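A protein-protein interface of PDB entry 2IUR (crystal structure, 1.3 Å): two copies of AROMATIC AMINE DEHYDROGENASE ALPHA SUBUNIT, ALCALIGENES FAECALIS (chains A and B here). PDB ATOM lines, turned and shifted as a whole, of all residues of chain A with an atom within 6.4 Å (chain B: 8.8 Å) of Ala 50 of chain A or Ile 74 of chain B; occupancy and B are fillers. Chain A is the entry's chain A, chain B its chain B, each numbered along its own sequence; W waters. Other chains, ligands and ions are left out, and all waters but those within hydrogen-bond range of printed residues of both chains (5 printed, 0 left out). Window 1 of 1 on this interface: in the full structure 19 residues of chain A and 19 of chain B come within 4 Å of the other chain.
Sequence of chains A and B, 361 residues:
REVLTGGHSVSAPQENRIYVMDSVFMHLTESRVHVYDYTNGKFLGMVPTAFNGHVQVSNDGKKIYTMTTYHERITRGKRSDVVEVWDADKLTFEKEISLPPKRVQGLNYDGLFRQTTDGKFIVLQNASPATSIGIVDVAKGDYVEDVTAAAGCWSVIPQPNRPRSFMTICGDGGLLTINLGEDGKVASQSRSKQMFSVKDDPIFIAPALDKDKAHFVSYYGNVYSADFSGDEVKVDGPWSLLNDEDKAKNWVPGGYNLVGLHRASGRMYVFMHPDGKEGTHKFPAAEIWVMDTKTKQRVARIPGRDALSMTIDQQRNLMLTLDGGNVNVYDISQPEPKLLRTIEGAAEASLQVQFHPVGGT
ND1 of His 27 of chain A is in hydrogen-bond range of OE2 of Glu 30 of chain B. The side-chain carboxylate of Glu 30 of chain B lies within hydrogen-bond range of the backbone NH of Leu 28 of chain A (3.3 Å). The side-chain hydroxyl (OG1) of Thr 29 of chain A lies within hydrogen-bond range of the side-chain carboxylate (OE1) of Glu 30 of chain B (2.6 Å). The side-chain carboxylate of Glu 30 of chain A sits at hydrogen-bond distance from the backbone NH of Leu 28 of chain B (3.3 Å). The side-chain carboxylate (OE1) of Glu 30 of chain A sits at hydrogen-bond distance from the side-chain hydroxyl (OG1) of Thr 29 of chain B (2.6 Å).
N of Asn 52 of chain A sits at hydrogen-bond distance from O of Leu 28 of chain A. The backbone carbonyl oxygen (O) of Tyr 70 of chain B sits at hydrogen-bond distance from the backbone NH (N) of Ser 80 of chain B (2.8 Å). OE2 of Glu 30 of chain A is in salt-bridge range of NH2 of Arg 32 of chain A, 2.8 Å away. The side-chain hydroxyl of Ser 31 of chain A lies within hydrogen-bond range of the backbone carbonyl oxygen of Ala 50 of chain A (2.7 Å).
Pro 48 of chain A touches Thr 75 of chain B. Ile 74 of chain B touches Ala 50 of chain A. Tyr 70 of chain A touches Arg 73 of chain B (CD1 to CD, 3.5 Å). Ile 74 of chain B touches Tyr 70 of chain A. Ala 50 of chain B touches Ile 74 of chain A. CD1 of Ile 74 of chain A touches CD2 of Tyr 70 of chain B, 3.9 Å away.
Of the printed residues of chain B, Leu 28 of chain A touches Glu 30 (3.3 Å). Ala 50 of chain A touches one residue of chain B. Thr 69 of chain A touches none of the printed residues of chain B. Printed residues of chain B within 4 Å of Ile 74 of chain A: Ala 50 (3.7 Å) and Tyr 70 (3.9 Å). Of the printed residues of chain A, Leu 28 of chain B touches Glu 30. Printed residues of chain A within 4 Å of Glu 30 of chain B: His 27, Leu 28 and Thr 29. Ile 74 of chain B touches two residues of chain A.
Of the 18 printed residues of chain A, 8 touch a printed residue of chain B. Hydrophobic or aromatic side chains of chain A that line the printed part of chain B: His 27, Pro 48, Ala 50, Tyr 70 and Ile 74. Among the printed residues, 11 pairs touch across the chains.
Leu 28 of chain A touches Glu 30 of chain B, and with the chains exchanged Glu 30 of chain A touches Leu 28 of chain B. Thr 29 of chain A touches Glu 30 of chain B, and with the chains exchanged Glu 30 of chain A touches Thr 29 of chain B. Ala 50 of chain A touches Ile 74 of chain B, and with the chains exchanged Ile 74 of chain A touches Ala 50 of chain B. Tyr 70 of chain A touches Ile 74 of chain B, and with the chains exchanged Ile 74 of chain A touches Tyr 70 of chain B. Positions printed for both chains: 28, 29, 30, 50, 51, 69, 70, 71 and 74. Of the 11 pairs that touch across the chains among the printed residues, 8 have their exchanged pair printed and touching as well.
Water W1 lies within hydrogen-bond range of OH of Tyr 70 of chain A (2.5 Å), O of Arg 73 of chain B (2.6 Å) and OG1 of Thr 75 of chain B (3.1 Å). Water W4 bridges O of Thr 29 of chain B (2.7 Å) and OG1 of Thr 29 of chain A (2.8 Å). Water W3 bridges the backbone carbonyl oxygen of Thr 29 of chain A and the side-chain hydroxyl of Thr 29 of chain B. Water W2 lies within hydrogen-bond range of the guanidinium group of Arg 76 of chain B (2.9 Å) and the side-chain hydroxyl of Tyr 70 of chain A (3.3 Å). Water W5 bridges O of His 71 of chain B and O of His 71 of chain A.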
ATOM      1  N   SER A  23      -5.859  -9.317  17.657  1.00  0.00           N
ATOM      2  CA  SER A  23      -6.723  -9.251  18.831  1.00  0.00           C
ATOM      3  C   SER A  23      -6.120  -9.977  20.001  1.00  0.00           C
ATOM      4  O   SER A  23      -6.429  -9.655  21.148  1.00  0.00           O
ATOM      5  CB  SER A  23      -8.110  -9.843  18.541  1.00  0.00           C
ATOM      6  OG  SER A  23      -8.102 -11.263  18.515  1.00  0.00           O
ATOM      7  N   HIS A  27      -5.474 -13.512  25.153  1.00  0.00           N
ATOM      8  CA  HIS A  27      -4.963 -12.532  26.100  1.00  0.00           C
ATOM      9  C   HIS A  27      -5.376 -11.167  25.595  1.00  0.00           C
ATOM     10  O   HIS A  27      -4.527 -10.296  25.320  1.00  0.00           O
ATOM     11  CB  HIS A  27      -3.454 -12.680  26.260  1.00  0.00           C
ATOM     12  CG  HIS A  27      -3.064 -13.992  26.822  1.00  0.00           C
ATOM     13  ND1 HIS A  27      -3.411 -14.369  28.102  1.00  0.00           N
ATOM     14  CD2 HIS A  27      -2.517 -15.075  26.237  1.00  0.00           C
ATOM     15  CE1 HIS A  27      -3.029 -15.625  28.296  1.00  0.00           C
ATOM     16  NE2 HIS A  27      -2.519 -16.086  27.168  1.00  0.00           N
ATOM     17  N   LEU A  28      -6.683 -10.936  25.574  1.00  0.00           N
ATOM     18  CA  LEU A  28      -7.285  -9.865  24.812  1.00  0.00           C
ATOM     19  C   LEU A  28      -6.955  -8.490  25.384  1.00  0.00           C
ATOM     20  O   LEU A  28      -7.162  -7.468  24.700  1.00  0.00           O
ATOM     21  CB  LEU A  28      -8.805 -10.083  24.772  1.00  0.00           C
ATOM     22  CG  LEU A  28      -9.673  -9.160  23.919  1.00  0.00           C
ATOM     23  CD1 LEU A  28      -9.199  -9.044  22.455  1.00  0.00           C
ATOM     24  CD2 LEU A  28     -11.152  -9.641  23.951  1.00  0.00           C
ATOM     25  N   THR A  29      -6.488  -8.412  26.634  1.00  0.00           N
ATOM     26  CA  THR A  29      -5.983  -7.141  27.182  1.00  0.00           C
ATOM     27  C   THR A  29      -4.640  -6.706  26.607  1.00  0.00           C
ATOM     28  O   THR A  29      -4.173  -5.606  26.927  1.00  0.00           O
ATOM     29  CB  THR A  29      -5.886  -7.113  28.703  1.00  0.00           C
ATOM     30  OG1 THR A  29      -4.915  -8.065  29.164  1.00  0.00           O
ATOM     31  CG2 THR A  29      -7.201  -7.458  29.364  1.00  0.00           C
ATOM     32  N   GLU A  30      -3.986  -7.559  25.799  1.00  0.00           N
ATOM     33  CA  GLU A  30      -2.695  -7.218  25.192  1.00  0.00           C
ATOM     34  C   GLU A  30      -2.785  -7.365  23.668  1.00  0.00           C
ATOM     35  O   GLU A  30      -1.812  -7.711  23.000  1.00  0.00           O
ATOM     36  CB  GLU A  30      -1.536  -8.028  25.777  1.00  0.00           C
ATOM     37  CG  GLU A  30      -0.212  -7.269  25.684  1.00  0.00           C
ATOM     38  CD  GLU A  30       0.985  -8.120  26.011  1.00  0.00           C
ATOM     39  OE1 GLU A  30       1.404  -8.157  27.201  1.00  0.00           O
ATOM     40  OE2 GLU A  30       1.567  -8.680  25.073  1.00  0.00           O
ATOM     41  N   SER A  31      -3.889  -6.871  23.124  1.00  0.00           N
ATOM     42  CA  SER A  31      -4.022  -6.746  21.676  1.00  0.00           C
ATOM     43  C   SER A  31      -3.001  -5.729  21.151  1.00  0.00           C
ATOM     44  O   SER A  31      -2.514  -4.888  21.893  1.00  0.00           O
ATOM     45  CB  SER A  31      -5.457  -6.318  21.308  1.00  0.00           C
ATOM     46  OG  SER A  31      -5.722  -4.940  21.632  1.00  0.00           O
ATOM     47  N   ARG A  32      -2.650  -5.836  19.884  1.00  0.00           N
ATOM     48  CA  ARG A  32      -1.692  -4.911  19.293  1.00  0.00           C
ATOM     49  C   ARG A  32      -1.801  -4.947  17.800  1.00  0.00           C
ATOM     50  O   ARG A  32      -2.348  -5.879  17.217  1.00  0.00           O
ATOM     51  CB  ARG A  32      -0.241  -5.275  19.720  1.00  0.00           C
ATOM     52  CG  ARG A  32       0.341  -6.590  19.073  1.00  0.00           C
ATOM     53  CD  ARG A  32      -0.036  -7.895  19.808  1.00  0.00           C
ATOM     54  NE  ARG A  32       0.612  -7.967  21.118  1.00  0.00           N
ATOM     55  CZ  ARG A  32       1.919  -8.215  21.288  1.00  0.00           C
ATOM     56  NH1 ARG A  32       2.719  -8.401  20.266  1.00  0.00           N
ATOM     57  NH2 ARG A  32       2.429  -8.178  22.501  1.00  0.00           N
ATOM     58  N   PRO A  48       0.979  -1.035  20.708  1.00  0.00           N
ATOM     59  CA  PRO A  48       0.137  -1.720  21.717  1.00  0.00           C
ATOM     60  C   PRO A  48      -1.239  -1.110  21.775  1.00  0.00           C
ATOM     61  O   PRO A  48      -1.352   0.117  21.710  1.00  0.00           O
ATOM     62  CB  PRO A  48       0.892  -1.454  23.023  1.00  0.00           C
ATOM     63  CG  PRO A  48       1.594  -0.144  22.796  1.00  0.00           C
ATOM     64  CD  PRO A  48       1.993  -0.161  21.337  1.00  0.00           C
ATOM     65  N   THR A  49      -2.292  -1.942  21.914  1.00  0.00           N
ATOM     66  CA  THR A  49      -3.662  -1.428  21.921  1.00  0.00           C
ATOM     67  C   THR A  49      -4.553  -2.029  23.020  1.00  0.00           C
ATOM     68  O   THR A  49      -5.766  -2.023  22.888  1.00  0.00           O
ATOM     69  CB  THR A  49      -4.337  -1.621  20.548  1.00  0.00           C
ATOM     70  OG1 THR A  49      -4.347  -3.003  20.165  1.00  0.00           O
ATOM     71  CG2 THR A  49      -3.599  -0.899  19.428  1.00  0.00           C
ATOM     72  N   ALA A  50      -3.954  -2.431  24.148  1.00  0.00           N
ATOM     73  CA  ALA A  50      -4.698  -2.766  25.358  1.00  0.00           C
ATOM     74  C   ALA A  50      -5.861  -3.746  25.059  1.00  0.00           C
ATOM     75  O   ALA A  50      -5.675  -4.719  24.326  1.00  0.00           O
ATOM     76  CB  ALA A  50      -5.141  -1.499  26.081  1.00  0.00           C
ATOM     77  N   PHE A  51      -7.065  -3.499  25.611  1.00  0.00           N
ATOM     78  CA  PHE A  51      -8.148  -4.454  25.500  1.00  0.00           C
ATOM     79  C   PHE A  51      -8.864  -4.253  24.171  1.00  0.00           C
ATOM     80  O   PHE A  51      -9.507  -3.241  23.956  1.00  0.00           O
ATOM     81  CB  PHE A  51      -9.145  -4.298  26.654  1.00  0.00           C
ATOM     82  CG  PHE A  51     -10.298  -5.279  26.585  1.00  0.00           C
ATOM     83  CD1 PHE A  51     -10.130  -6.624  26.917  1.00  0.00           C
ATOM     84  CD2 PHE A  51     -11.547  -4.848  26.189  1.00  0.00           C
ATOM     85  CE1 PHE A  51     -11.186  -7.526  26.821  1.00  0.00           C
ATOM     86  CE2 PHE A  51     -12.628  -5.779  26.120  1.00  0.00           C
ATOM     87  CZ  PHE A  51     -12.427  -7.090  26.451  1.00  0.00           C
ATOM     88  N   ASN A  52      -8.883  -5.298  23.340  1.00  0.00           N
ATOM     89  CA  ASN A  52      -9.647  -5.311  22.084  1.00  0.00           C
ATOM     90  C   ASN A  52      -9.476  -4.033  21.294  1.00  0.00           C
ATOM     91  O   ASN A  52     -10.450  -3.329  20.985  1.00  0.00           O
ATOM     92  CB  ASN A  52     -11.133  -5.534  22.393  1.00  0.00           C
ATOM     93  CG  ASN A  52     -11.998  -5.592  21.139  1.00  0.00           C
ATOM     94  OD1 ASN A  52     -11.622  -6.172  20.069  1.00  0.00           O
ATOM     95  ND2 ASN A  52     -13.147  -4.985  21.228  1.00  0.00           N
ATOM     96  N   GLY A  53      -8.268  -3.739  20.906  1.00  0.00           N
ATOM     97  CA  GLY A  53      -8.022  -2.553  20.135  1.00  0.00           C
ATOM     98  C   GLY A  53      -8.541  -2.647  18.717  1.00  0.00           C
ATOM     99  O   GLY A  53      -8.730  -3.728  18.167  1.00  0.00           O
ATOM    100  N   THR A  68      -9.461   1.951  21.961  1.00  0.00           N
ATOM    101  CA  THR A  68      -9.300   0.912  22.959  1.00  0.00           C
ATOM    102  C   THR A  68      -9.957   1.313  24.257  1.00  0.00           C
ATOM    103  O   THR A  68     -10.560   2.377  24.359  1.00  0.00           O
ATOM    104  CB  THR A  68      -7.828   0.557  23.134  1.00  0.00           C
ATOM    105  OG1 THR A  68      -7.735  -0.614  23.978  1.00  0.00           O
ATOM    106  CG2 THR A  68      -7.037   1.663  23.847  1.00  0.00           C
ATOM    107  N   THR A  69      -9.955   0.362  25.194  1.00  0.00           N
ATOM    108  CA  THR A  69     -10.485   0.557  26.545  1.00  0.00           C
ATOM    109  C   THR A  69      -9.409   0.246  27.556  1.00  0.00           C
ATOM    110  O   THR A  69      -8.720  -0.772  27.457  1.00  0.00           O
ATOM    111  CB  THR A  69     -11.660  -0.406  26.760  1.00  0.00           C
ATOM    112  OG1 THR A  69     -12.759  -0.034  25.902  1.00  0.00           O
ATOM    113  CG2 THR A  69     -12.201  -0.346  28.230  1.00  0.00           C
ATOM    114  N   TYR A  70      -9.238   1.160  28.516  1.00  0.00           N
ATOM    115  CA  TYR A  70      -8.403   0.958  29.706  1.00  0.00           C
ATOM    116  C   TYR A  70      -9.298   0.940  30.945  1.00  0.00           C
ATOM    117  O   TYR A  70     -10.403   1.485  30.938  1.00  0.00           O
ATOM    118  CB  TYR A  70      -7.438   2.133  29.877  1.00  0.00           C
ATOM    119  CG  TYR A  70      -6.442   2.304  28.776  1.00  0.00           C
ATOM    120  CD1 TYR A  70      -6.682   3.192  27.750  1.00  0.00           C
ATOM    121  CD2 TYR A  70      -5.250   1.597  28.756  1.00  0.00           C
ATOM    122  CE1 TYR A  70      -5.766   3.363  26.717  1.00  0.00           C
ATOM    123  CE2 TYR A  70      -4.324   1.770  27.737  1.00  0.00           C
ATOM    124  CZ  TYR A  70      -4.593   2.667  26.725  1.00  0.00           C
ATOM    125  OH  TYR A  70      -3.669   2.868  25.727  1.00  0.00           O
ATOM    126  N   HIS A  71      -8.798   0.319  32.015  1.00  0.00           N
ATOM    127  CA  HIS A  71      -9.327   0.536  33.364  1.00  0.00           C
ATOM    128  C   HIS A  71      -8.155   0.783  34.288  1.00  0.00           C
ATOM    129  O   HIS A  71      -7.063   0.297  34.069  1.00  0.00           O
ATOM    130  CB  HIS A  71     -10.121  -0.688  33.868  1.00  0.00           C
ATOM    131  CG  HIS A  71     -11.317  -1.032  33.037  1.00  0.00           C
ATOM    132  ND1 HIS A  71     -12.613  -0.694  33.382  1.00  0.00           N
ATOM    133  CD2 HIS A  71     -11.411  -1.700  31.860  1.00  0.00           C
ATOM    134  CE1 HIS A  71     -13.444  -1.162  32.462  1.00  0.00           C
ATOM    135  NE2 HIS A  71     -12.735  -1.773  31.535  1.00  0.00           N
ATOM    136  N   ILE A  74      -7.163  -2.545  35.235  1.00  0.00           N
ATOM    137  CA  ILE A  74      -7.447  -3.533  34.161  1.00  0.00           C
ATOM    138  C   ILE A  74      -8.775  -4.245  34.328  1.00  0.00           C
ATOM    139  O   ILE A  74      -9.697  -4.048  33.524  1.00  0.00           O
ATOM    140  CB  ILE A  74      -6.275  -4.518  33.994  1.00  0.00           C
ATOM    141  CG1 ILE A  74      -4.921  -3.778  33.818  1.00  0.00           C
ATOM    142  CG2 ILE A  74      -6.513  -5.392  32.771  1.00  0.00           C
ATOM    143  CD1 ILE A  74      -3.722  -4.652  33.936  1.00  0.00           C
ATOM    144  N   LEU B  28       3.104 -10.618  28.683  1.00  0.00           N
ATOM    145  CA  LEU B  28       3.462 -10.565  30.085  1.00  0.00           C
ATOM    146  C   LEU B  28       2.617  -9.587  30.884  1.00  0.00           C
ATOM    147  O   LEU B  28       2.621  -9.659  32.128  1.00  0.00           O
ATOM    148  CB  LEU B  28       4.957 -10.201  30.184  1.00  0.00           C
ATOM    149  CG  LEU B  28       5.637 -10.240  31.562  1.00  0.00           C
ATOM    150  CD1 LEU B  28       5.407 -11.535  32.307  1.00  0.00           C
ATOM    151  CD2 LEU B  28       7.136 -10.003  31.417  1.00  0.00           C
ATOM    152  N   THR B  29       1.907  -8.667  30.216  1.00  0.00           N
ATOM    153  CA  THR B  29       0.958  -7.795  30.908  1.00  0.00           C
ATOM    154  C   THR B  29      -0.323  -8.504  31.340  1.00  0.00           C
ATOM    155  O   THR B  29      -1.160  -7.890  32.001  1.00  0.00           O
ATOM    156  CB  THR B  29       0.579  -6.547  30.095  1.00  0.00           C
ATOM    157  OG1 THR B  29      -0.076  -6.933  28.887  1.00  0.00           O
ATOM    158  CG2 THR B  29       1.802  -5.731  29.726  1.00  0.00           C
ATOM    159  N   GLU B  30      -0.532  -9.767  30.911  1.00  0.00           N
ATOM    160  CA  GLU B  30      -1.736 -10.539  31.305  1.00  0.00           C
ATOM    161  C   GLU B  30      -1.338 -11.831  31.985  1.00  0.00           C
ATOM    162  O   GLU B  30      -1.968 -12.866  31.783  1.00  0.00           O
ATOM    163  CB  GLU B  30      -2.659 -10.803  30.108  1.00  0.00           C
ATOM    164  CG  GLU B  30      -4.130 -10.909  30.528  1.00  0.00           C
ATOM    165  CD  GLU B  30      -5.001 -11.399  29.420  1.00  0.00           C
ATOM    166  OE1 GLU B  30      -5.584 -10.559  28.690  1.00  0.00           O
ATOM    167  OE2 GLU B  30      -5.196 -12.611  29.308  1.00  0.00           O
ATOM    168  N   ALA B  50      -1.821  -8.917  36.051  1.00  0.00           N
ATOM    169  CA  ALA B  50      -1.232  -7.813  35.290  1.00  0.00           C
ATOM    170  C   ALA B  50       0.202  -8.136  34.859  1.00  0.00           C
ATOM    171  O   ALA B  50       0.439  -9.208  34.328  1.00  0.00           O
ATOM    172  CB  ALA B  50      -1.318  -6.511  36.078  1.00  0.00           C
ATOM    173  N   PHE B  51       1.131  -7.177  34.976  1.00  0.00           N
ATOM    174  CA  PHE B  51       2.465  -7.350  34.425  1.00  0.00           C
ATOM    175  C   PHE B  51       3.349  -8.133  35.374  1.00  0.00           C
ATOM    176  O   PHE B  51       3.648  -7.660  36.480  1.00  0.00           O
ATOM    177  CB  PHE B  51       3.116  -6.007  34.128  1.00  0.00           C
ATOM    178  CG  PHE B  51       4.505  -6.119  33.574  1.00  0.00           C
ATOM    179  CD1 PHE B  51       4.716  -6.455  32.249  1.00  0.00           C
ATOM    180  CD2 PHE B  51       5.613  -5.860  34.377  1.00  0.00           C
ATOM    181  CE1 PHE B  51       5.999  -6.550  31.735  1.00  0.00           C
ATOM    182  CE2 PHE B  51       6.903  -5.955  33.848  1.00  0.00           C
ATOM    183  CZ  PHE B  51       7.075  -6.282  32.527  1.00  0.00           C
ATOM    184  N   THR B  69       2.662  -4.922  38.949  1.00  0.00           N
ATOM    185  CA  THR B  69       2.887  -3.541  38.490  1.00  0.00           C
ATOM    186  C   THR B  69       1.787  -3.154  37.521  1.00  0.00           C
ATOM    187  O   THR B  69       1.486  -3.895  36.578  1.00  0.00           O
ATOM    188  CB  THR B  69       4.238  -3.412  37.787  1.00  0.00           C
ATOM    189  OG1 THR B  69       5.302  -3.624  38.721  1.00  0.00           O
ATOM    190  CG2 THR B  69       4.457  -1.988  37.234  1.00  0.00           C
ATOM    191  N   TYR B  70       1.156  -2.017  37.796  1.00  0.00           N
ATOM    192  CA  TYR B  70       0.241  -1.338  36.876  1.00  0.00           C
ATOM    193  C   TYR B  70       0.882  -0.042  36.378  1.00  0.00           C
ATOM    194  O   TYR B  70       1.726   0.566  37.055  1.00  0.00           O
ATOM    195  CB  TYR B  70      -1.087  -0.982  37.577  1.00  0.00           C
ATOM    196  CG  TYR B  70      -1.859  -2.160  38.118  1.00  0.00           C
ATOM    197  CD1 TYR B  70      -1.711  -2.566  39.439  1.00  0.00           C
ATOM    198  CD2 TYR B  70      -2.733  -2.880  37.316  1.00  0.00           C
ATOM    199  CE1 TYR B  70      -2.425  -3.627  39.941  1.00  0.00           C
ATOM    200  CE2 TYR B  70      -3.467  -3.956  37.818  1.00  0.00           C
ATOM    201  CZ  TYR B  70      -3.273  -4.340  39.123  1.00  0.00           C
ATOM    202  OH  TYR B  70      -4.032  -5.395  39.641  1.00  0.00           O
ATOM    203  N   HIS B  71       0.431   0.410  35.218  1.00  0.00           N
ATOM    204  CA  HIS B  71       0.586   1.819  34.850  1.00  0.00           C
ATOM    205  C   HIS B  71      -0.762   2.360  34.387  1.00  0.00           C
ATOM    206  O   HIS B  71      -1.600   1.610  33.864  1.00  0.00           O
ATOM    207  CB  HIS B  71       1.640   2.044  33.740  1.00  0.00           C
ATOM    208  CG  HIS B  71       3.017   1.561  34.076  1.00  0.00           C
ATOM    209  ND1 HIS B  71       4.055   2.398  34.427  1.00  0.00           N
ATOM    210  CD2 HIS B  71       3.532   0.309  34.079  1.00  0.00           C
ATOM    211  CE1 HIS B  71       5.150   1.675  34.621  1.00  0.00           C
ATOM    212  NE2 HIS B  71       4.847   0.407  34.436  1.00  0.00           N
ATOM    213  N   GLU B  72      -0.912   3.681  34.453  1.00  0.00           N
ATOM    214  CA  GLU B  72      -2.197   4.284  34.139  1.00  0.00           C
ATOM    215  C   GLU B  72      -2.700   3.920  32.740  1.00  0.00           C
ATOM    216  O   GLU B  72      -3.912   3.754  32.524  1.00  0.00           O
ATOM    217  CB  GLU B  72      -2.138   5.808  34.248  1.00  0.00           C
ATOM    218  CG  GLU B  72      -1.739   6.379  35.599  1.00  0.00           C
ATOM    219  CD  GLU B  72      -1.539   7.918  35.577  1.00  0.00           C
ATOM    220  OE1 GLU B  72      -0.681   8.433  34.798  1.00  0.00           O
ATOM    221  OE2 GLU B  72      -2.215   8.622  36.374  1.00  0.00           O
ATOM    222  N   ARG B  73      -1.768   3.795  31.794  1.00  0.00           N
ATOM    223  CA  ARG B  73      -2.111   3.445  30.452  1.00  0.00           C
ATOM    224  C   ARG B  73      -1.224   2.295  29.951  1.00  0.00           C
ATOM    225  O   ARG B  73      -0.945   2.181  28.742  1.00  0.00           O
ATOM    226  CB  ARG B  73      -1.981   4.673  29.547  1.00  0.00           C
ATOM    227  CG  ARG B  73      -3.031   5.717  29.816  1.00  0.00           C
ATOM    228  CD  ARG B  73      -4.399   5.312  29.296  1.00  0.00           C
ATOM    229  NE  ARG B  73      -5.388   6.379  29.402  1.00  0.00           N
ATOM    230  CZ  ARG B  73      -6.143   6.591  30.444  1.00  0.00           C
ATOM    231  NH1 ARG B  73      -6.108   5.790  31.490  1.00  0.00           N
ATOM    232  NH2 ARG B  73      -6.987   7.612  30.430  1.00  0.00           N
ATOM    233  N   ILE B  74      -0.839   1.424  30.893  1.00  0.00           N
ATOM    234  CA  ILE B  74      -0.106   0.163  30.651  1.00  0.00           C
ATOM    235  C   ILE B  74       1.354   0.392  30.215  1.00  0.00           C
ATOM    236  O   ILE B  74       2.291   0.073  30.951  1.00  0.00           O
ATOM    237  CB  ILE B  74      -0.849  -0.786  29.677  1.00  0.00           C
ATOM    238  CG1 ILE B  74      -2.303  -1.004  30.120  1.00  0.00           C
ATOM    239  CG2 ILE B  74      -0.088  -2.140  29.634  1.00  0.00           C
ATOM    240  CD1 ILE B  74      -3.111  -1.734  29.127  1.00  0.00           C
ATOM    241  N   THR B  75       1.533   0.914  29.001  1.00  0.00           N
ATOM    242  CA  THR B  75       2.835   1.160  28.429  1.00  0.00           C
ATOM    243  C   THR B  75       3.272   2.645  28.593  1.00  0.00           C
ATOM    244  O   THR B  75       4.342   3.034  28.141  1.00  0.00           O
ATOM    245  CB  THR B  75       2.848   0.776  26.962  1.00  0.00           C
ATOM    246  OG1 THR B  75       1.661   1.278  26.320  1.00  0.00           O
ATOM    247  CG2 THR B  75       2.809  -0.735  26.787  1.00  0.00           C
ATOM    248  N   ARG B  76       2.416   3.453  29.209  1.00  0.00           N
ATOM    249  CA  ARG B  76       2.780   4.811  29.592  1.00  0.00           C
ATOM    250  C   ARG B  76       1.956   5.193  30.824  1.00  0.00           C
ATOM    251  O   ARG B  76       1.031   4.478  31.223  1.00  0.00           O
ATOM    252  CB  ARG B  76       2.514   5.799  28.439  1.00  0.00           C
ATOM    253  CG  ARG B  76       1.077   5.900  28.041  1.00  0.00           C
ATOM    254  CD  ARG B  76       0.809   6.688  26.762  1.00  0.00           C
ATOM    255  NE  ARG B  76      -0.570   6.560  26.332  1.00  0.00           N
ATOM    256  CZ  ARG B  76      -1.581   7.293  26.764  1.00  0.00           C
ATOM    257  NH1 ARG B  76      -1.364   8.273  27.618  1.00  0.00           N
ATOM    258  NH2 ARG B  76      -2.812   7.027  26.362  1.00  0.00           N
ATOM    259  N   GLY B  77       2.328   6.302  31.435  1.00  0.00           N
ATOM    260  CA  GLY B  77       1.616   6.802  32.614  1.00  0.00           C
ATOM    261  C   GLY B  77       2.245   6.331  33.905  1.00  0.00           C
ATOM    262  O   GLY B  77       3.224   5.584  33.911  1.00  0.00           O
ATOM    263  N   LYS B  78       1.680   6.795  35.014  1.00  0.00           N
ATOM    264  CA  LYS B  78       2.277   6.582  36.317  1.00  0.00           C
ATOM    265  C   LYS B  78       2.269   5.104  36.706  1.00  0.00           C
ATOM    266  O   LYS B  78       1.279   4.409  36.497  1.00  0.00           O
ATOM    267  CB  LYS B  78       1.543   7.385  37.379  1.00  0.00           C
ATOM    268  CG  LYS B  78       2.246   7.344  38.738  1.00  0.00           C
ATOM    269  CD  LYS B  78       1.547   8.188  39.786  1.00  0.00           C
ATOM    270  CE  LYS B  78       2.332   8.192  41.103  1.00  0.00           C
ATOM    271  NZ  LYS B  78       1.596   8.894  42.182  1.00  0.00           N
ATOM    272  N   ARG B  79       3.408   4.672  37.249  1.00  0.00           N
ATOM    273  CA  ARG B  79       3.601   3.318  37.769  1.00  0.00           C
ATOM    274  C   ARG B  79       3.015   3.153  39.153  1.00  0.00           C
ATOM    275  O   ARG B  79       3.213   4.018  40.029  1.00  0.00           O
ATOM    276  CB  ARG B  79       5.078   3.025  37.835  1.00  0.00           C
ATOM    277  CG  ARG B  79       5.462   1.634  38.344  1.00  0.00           C
ATOM    278  CD  ARG B  79       6.889   1.275  38.016  1.00  0.00           C
ATOM    279  NE  ARG B  79       7.375   0.101  38.731  1.00  0.00           N
ATOM    280  CZ  ARG B  79       8.574  -0.410  38.589  1.00  0.00           C
ATOM    281  NH1 ARG B  79       9.426   0.126  37.727  1.00  0.00           N
ATOM    282  NH2 ARG B  79       8.965  -1.438  39.330  1.00  0.00           N
ATOM    283  N   SER B  80       2.337   2.032  39.366  1.00  0.00           N
ATOM    284  CA  SER B  80       1.907   1.613  40.710  1.00  0.00           C
ATOM    285  C   SER B  80       2.305   0.171  40.942  1.00  0.00           C
ATOM    286  O   SER B  80       1.695  -0.737  40.333  1.00  0.00           O
ATOM    287  CB  SER B  80       0.390   1.713  40.871  1.00  0.00           C
ATOM    288  OG  SER B  80      -0.093   3.042  40.724  1.00  0.00           O
HETATM  289  O   HOH W   1      -1.244   2.232  26.128  1.00  0.00           O
HETATM  290  O   HOH W   2      -0.798   4.163  24.687  1.00  0.00           O
HETATM  291  O   HOH W   3      -1.776  -4.860  28.023  1.00  0.00           O
HETATM  292  O   HOH W   4      -3.828  -7.442  31.637  1.00  0.00           O
HETATM  293  O   HOH W   5      -4.068  -0.083  33.452  1.00  0.00           O
